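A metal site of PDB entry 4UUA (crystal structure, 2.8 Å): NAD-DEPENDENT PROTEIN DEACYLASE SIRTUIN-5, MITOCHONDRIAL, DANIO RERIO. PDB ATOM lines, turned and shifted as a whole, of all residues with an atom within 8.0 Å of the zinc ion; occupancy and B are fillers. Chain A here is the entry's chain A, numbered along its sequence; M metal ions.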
ATOM      1  N   ARG A 138      24.668 -13.506  -1.284  1.00  0.00           N
ATOM      2  CA  ARG A 138      23.272 -13.093  -1.314  1.00  0.00           C
ATOM      3  C   ARG A 138      22.867 -12.382  -0.028  1.00  0.00           C
ATOM      4  O   ARG A 138      23.200 -12.818   1.051  1.00  0.00           O
ATOM      5  CB  ARG A 138      22.401 -14.309  -1.514  1.00  0.00           C
ATOM      6  CG  ARG A 138      21.089 -13.928  -2.135  1.00  0.00           C
ATOM      7  CD  ARG A 138      20.452 -15.132  -2.762  1.00  0.00           C
ATOM      8  NE  ARG A 138      19.891 -16.081  -1.816  1.00  0.00           N
ATOM      9  CZ  ARG A 138      20.296 -17.321  -1.614  1.00  0.00           C
ATOM     10  NH1 ARG A 138      21.321 -17.834  -2.273  1.00  0.00           N
ATOM     11  NH2 ARG A 138      19.661 -18.054  -0.716  1.00  0.00           N
ATOM     12  N   CYS A 139      22.147 -11.272  -0.144  1.00  0.00           N
ATOM     13  CA  CYS A 139      21.847 -10.471   1.002  1.00  0.00           C
ATOM     14  C   CYS A 139      20.645 -11.085   1.645  1.00  0.00           C
ATOM     15  O   CYS A 139      19.598 -11.177   1.021  1.00  0.00           O
ATOM     16  CB  CYS A 139      21.556  -9.032   0.615  1.00  0.00           C
ATOM     17  SG  CYS A 139      21.057  -7.975   1.984  1.00  0.00           S
ATOM     18  N   MET A 140      20.781 -11.507   2.888  1.00  0.00           N
ATOM     19  CA  MET A 140      19.662 -12.026   3.600  1.00  0.00           C
ATOM     20  C   MET A 140      18.523 -11.018   3.566  1.00  0.00           C
ATOM     21  O   MET A 140      17.371 -11.389   3.746  1.00  0.00           O
ATOM     22  CB  MET A 140      20.021 -12.319   5.068  1.00  0.00           C
ATOM     23  CG  MET A 140      20.999 -13.454   5.291  1.00  0.00           C
ATOM     24  SD  MET A 140      20.472 -15.028   4.648  1.00  0.00           S
ATOM     25  CE  MET A 140      19.208 -15.548   5.813  1.00  0.00           C
ATOM     26  N   SER A 141      18.802  -9.740   3.385  1.00  0.00           N
ATOM     27  CA  SER A 141      17.743  -8.749   3.596  1.00  0.00           C
ATOM     28  C   SER A 141      17.103  -8.352   2.317  1.00  0.00           C
ATOM     29  O   SER A 141      15.922  -8.526   2.202  1.00  0.00           O
ATOM     30  CB  SER A 141      18.222  -7.526   4.339  1.00  0.00           C
ATOM     31  OG  SER A 141      17.130  -6.823   4.807  1.00  0.00           O
ATOM     32  N   CYS A 142      17.867  -7.855   1.335  1.00  0.00           N
ATOM     33  CA  CYS A 142      17.291  -7.466   0.025  1.00  0.00           C
ATOM     34  C   CYS A 142      17.444  -8.473  -1.112  1.00  0.00           C
ATOM     35  O   CYS A 142      16.907  -8.291  -2.190  1.00  0.00           O
ATOM     36  CB  CYS A 142      17.856  -6.099  -0.411  1.00  0.00           C
ATOM     37  SG  CYS A 142      19.588  -6.042  -0.903  1.00  0.00           S
ATOM     38  N   GLY A 143      18.186  -9.543  -0.894  1.00  0.00           N
ATOM     39  CA  GLY A 143      18.364 -10.583  -1.908  1.00  0.00           C
ATOM     40  C   GLY A 143      19.259 -10.232  -3.089  1.00  0.00           C
ATOM     41  O   GLY A 143      19.291 -10.975  -4.070  1.00  0.00           O
ATOM     42  N   GLU A 144      20.024  -9.144  -2.994  1.00  0.00           N
ATOM     43  CA  GLU A 144      20.982  -8.836  -4.071  1.00  0.00           C
ATOM     44  C   GLU A 144      22.070  -9.926  -4.189  1.00  0.00           C
ATOM     45  O   GLU A 144      22.600 -10.400  -3.191  1.00  0.00           O
ATOM     46  CB  GLU A 144      21.632  -7.462  -3.888  1.00  0.00           C
ATOM     47  CG  GLU A 144      22.733  -7.165  -4.890  1.00  0.00           C
ATOM     48  CD  GLU A 144      23.327  -5.784  -4.728  1.00  0.00           C
ATOM     49  OE1 GLU A 144      22.581  -4.798  -4.873  1.00  0.00           O
ATOM     50  OE2 GLU A 144      24.542  -5.673  -4.436  1.00  0.00           O
ATOM     51  N   VAL A 145      22.372 -10.337  -5.414  1.00  0.00           N
ATOM     52  CA  VAL A 145      23.354 -11.358  -5.659  1.00  0.00           C
ATOM     53  C   VAL A 145      24.502 -10.640  -6.296  1.00  0.00           C
ATOM     54  O   VAL A 145      24.376 -10.142  -7.394  1.00  0.00           O
ATOM     55  CB  VAL A 145      22.820 -12.448  -6.619  1.00  0.00           C
ATOM     56  CG1 VAL A 145      23.859 -13.543  -6.811  1.00  0.00           C
ATOM     57  CG2 VAL A 145      21.522 -13.036  -6.085  1.00  0.00           C
ATOM     58  N   ARG A 179      28.501  -7.600   5.261  1.00  0.00           N
ATOM     59  CA  ARG A 179      27.244  -6.931   5.172  1.00  0.00           C
ATOM     60  C   ARG A 179      27.069  -6.408   3.778  1.00  0.00           C
ATOM     61  O   ARG A 179      28.043  -6.157   3.078  1.00  0.00           O
ATOM     62  CB  ARG A 179      27.199  -5.766   6.127  1.00  0.00           C
ATOM     63  CG  ARG A 179      27.626  -6.055   7.557  1.00  0.00           C
ATOM     64  CD  ARG A 179      26.793  -7.125   8.239  1.00  0.00           C
ATOM     65  NE  ARG A 179      25.359  -6.847   8.238  1.00  0.00           N
ATOM     66  CZ  ARG A 179      24.481  -7.412   9.068  1.00  0.00           C
ATOM     67  NH1 ARG A 179      24.855  -8.263  10.011  1.00  0.00           N
ATOM     68  NH2 ARG A 179      23.210  -7.088   8.985  1.00  0.00           N
ATOM     69  N   CYS A 180      25.816  -6.226   3.399  1.00  0.00           N
ATOM     70  CA  CYS A 180      25.451  -5.764   2.063  1.00  0.00           C
ATOM     71  C   CYS A 180      25.685  -4.268   1.930  1.00  0.00           C
ATOM     72  O   CYS A 180      25.195  -3.498   2.738  1.00  0.00           O
ATOM     73  CB  CYS A 180      23.973  -6.108   1.796  1.00  0.00           C
ATOM     74  SG  CYS A 180      23.091  -5.181   0.538  1.00  0.00           S
ATOM     75  N   GLU A 181      26.388  -3.878   0.876  1.00  0.00           N
ATOM     76  CA  GLU A 181      26.975  -2.571   0.829  1.00  0.00           C
ATOM     77  C   GLU A 181      26.025  -1.472   0.514  1.00  0.00           C
ATOM     78  O   GLU A 181      26.335  -0.309   0.793  1.00  0.00           O
ATOM     79  CB  GLU A 181      28.192  -2.541  -0.083  1.00  0.00           C
ATOM     80  CG  GLU A 181      29.421  -3.166   0.565  1.00  0.00           C
ATOM     81  CD  GLU A 181      30.546  -3.263  -0.403  1.00  0.00           C
ATOM     82  OE1 GLU A 181      31.105  -2.202  -0.661  1.00  0.00           O
ATOM     83  OE2 GLU A 181      30.837  -4.343  -0.946  1.00  0.00           O
ATOM     84  N   ARG A 182      24.852  -1.787  -0.020  1.00  0.00           N
ATOM     85  CA  ARG A 182      23.813  -0.772  -0.177  1.00  0.00           C
ATOM     86  C   ARG A 182      23.413  -0.233   1.215  1.00  0.00           C
ATOM     87  O   ARG A 182      22.720  -0.917   1.968  1.00  0.00           O
ATOM     88  CB  ARG A 182      22.614  -1.346  -0.902  1.00  0.00           C
ATOM     89  CG  ARG A 182      22.929  -1.923  -2.278  1.00  0.00           C
ATOM     90  CD  ARG A 182      21.826  -2.859  -2.773  1.00  0.00           C
ATOM     91  NE  ARG A 182      20.564  -2.138  -3.094  1.00  0.00           N
ATOM     92  CZ  ARG A 182      19.471  -2.013  -2.294  1.00  0.00           C
ATOM     93  NH1 ARG A 182      19.406  -2.495  -1.051  1.00  0.00           N
ATOM     94  NH2 ARG A 182      18.422  -1.342  -2.746  1.00  0.00           N
ATOM     95  N   LYS A 183      23.893   0.948   1.562  1.00  0.00           N
ATOM     96  CA  LYS A 183      23.837   1.459   2.941  1.00  0.00           C
ATOM     97  C   LYS A 183      22.416   1.706   3.449  1.00  0.00           C
ATOM     98  O   LYS A 183      22.224   1.891   4.649  1.00  0.00           O
ATOM     99  CB  LYS A 183      24.638   2.758   3.095  1.00  0.00           C
ATOM    100  CG  LYS A 183      26.140   2.583   3.355  1.00  0.00           C
ATOM    101  CD  LYS A 183      26.906   3.880   3.137  1.00  0.00           C
ATOM    102  CE  LYS A 183      27.162   4.149   1.653  1.00  0.00           C
ATOM    103  NZ  LYS A 183      27.766   5.487   1.422  1.00  0.00           N
ATOM    104  N   SER A 184      21.447   1.772   2.544  1.00  0.00           N
ATOM    105  CA  SER A 184      20.040   1.785   2.935  1.00  0.00           C
ATOM    106  C   SER A 184      19.676   0.471   3.630  1.00  0.00           C
ATOM    107  O   SER A 184      18.801   0.461   4.493  1.00  0.00           O
ATOM    108  CB  SER A 184      19.152   1.993   1.715  1.00  0.00           C
ATOM    109  OG  SER A 184      19.596   1.206   0.616  1.00  0.00           O
ATOM    110  N   CYS A 185      20.363  -0.622   3.259  1.00  0.00           N
ATOM    111  CA  CYS A 185      20.011  -1.987   3.670  1.00  0.00           C
ATOM    112  C   CYS A 185      20.900  -2.550   4.770  1.00  0.00           C
ATOM    113  O   CYS A 185      20.421  -3.021   5.801  1.00  0.00           O
ATOM    114  CB  CYS A 185      20.036  -2.919   2.440  1.00  0.00           C
ATOM    115  SG  CYS A 185      20.097  -4.679   2.819  1.00  0.00           S
ATOM    116  N   ASN A 186      22.206  -2.531   4.519  1.00  0.00           N
ATOM    117  CA  ASN A 186      23.195  -3.117   5.427  1.00  0.00           C
ATOM    118  C   ASN A 186      22.882  -4.544   5.886  1.00  0.00           C
ATOM    119  O   ASN A 186      23.206  -4.911   6.983  1.00  0.00           O
ATOM    120  CB  ASN A 186      23.385  -2.220   6.614  1.00  0.00           C
ATOM    121  CG  ASN A 186      24.605  -2.609   7.425  1.00  0.00           C
ATOM    122  OD1 ASN A 186      25.681  -2.771   6.894  1.00  0.00           O
ATOM    123  ND2 ASN A 186      24.445  -2.711   8.734  1.00  0.00           N
ATOM    124  N   GLY A 187      22.254  -5.330   5.023  1.00  0.00           N
ATOM    125  CA  GLY A 187      21.775  -6.677   5.376  1.00  0.00           C
ATOM    126  C   GLY A 187      22.911  -7.639   5.492  1.00  0.00           C
ATOM    127  O   GLY A 187      23.988  -7.382   4.951  1.00  0.00           O
ATOM    128  N   LEU A 188      22.684  -8.740   6.208  1.00  0.00           N
ATOM    129  CA  LEU A 188      23.714  -9.773   6.412  1.00  0.00           C
ATOM    130  C   LEU A 188      23.938 -10.656   5.181  1.00  0.00           C
ATOM    131  O   LEU A 188      22.980 -11.184   4.632  1.00  0.00           O
ATOM    132  CB  LEU A 188      23.337 -10.661   7.580  1.00  0.00           C
ATOM    133  CG  LEU A 188      24.095 -11.983   7.667  1.00  0.00           C
ATOM    134  CD1 LEU A 188      25.570 -11.717   7.974  1.00  0.00           C
ATOM    135  CD2 LEU A 188      23.511 -12.898   8.718  1.00  0.00           C
ATOM    136  N   LEU A 189      25.168 -10.868   4.767  1.00  0.00           N
ATOM    137  CA  LEU A 189      25.376 -11.641   3.557  1.00  0.00           C
ATOM    138  C   LEU A 189      25.506 -13.100   3.879  1.00  0.00           C
ATOM    139  O   LEU A 189      25.955 -13.461   4.960  1.00  0.00           O
ATOM    140  CB  LEU A 189      26.599 -11.168   2.781  1.00  0.00           C
ATOM    141  CG  LEU A 189      26.535  -9.740   2.209  1.00  0.00           C
ATOM    142  CD1 LEU A 189      27.748  -9.462   1.334  1.00  0.00           C
ATOM    143  CD2 LEU A 189      25.270  -9.494   1.413  1.00  0.00           C
HETATM  144 ZN    ZN M   1      20.975  -5.860   0.992  1.00  0.00          ZN
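The backbone carbonyl oxygen (O) of Gly 187 sits at hydrogen-bond distance from the backbone NH (N) of Cys 180.
The guanidinium group of Arg 182 sits close to the side-chain sulfur of Cys 142 (3.6 Å).
The backbone NH (N) of Cys 139 is in hydrogen-bond range of the backbone carbonyl oxygen (O) of Glu 144 (3.2 Å).
The backbone NH of Ser 141 sits close to the side-chain sulfur of Cys 139 (3.2 Å).
The side-chain sulfur (SG) of Cys 185 sits close to the backbone NH (N) of Gly 187, 3.2 Å away.
The backbone NH (N) of Glu 144 sits close to the side-chain sulfur (SG) of Cys 142.
Of the 19 residues printed, 4 come within 4 Å of the zinc ion.
The nearest printed residue that does not touch the zinc ion is Arg 182 (4.2 Å).
The zinc ion is bound by the side-chain sulfur (SG) of Cys 180 (2.3 Å), the side-chain sulfur (SG) of Cys 139 (2.3 Å), the side-chain sulfur (SG) of Cys 185 (2.3 Å) and the side-chain sulfur (SG) of Cys 142 (2.4 Å).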
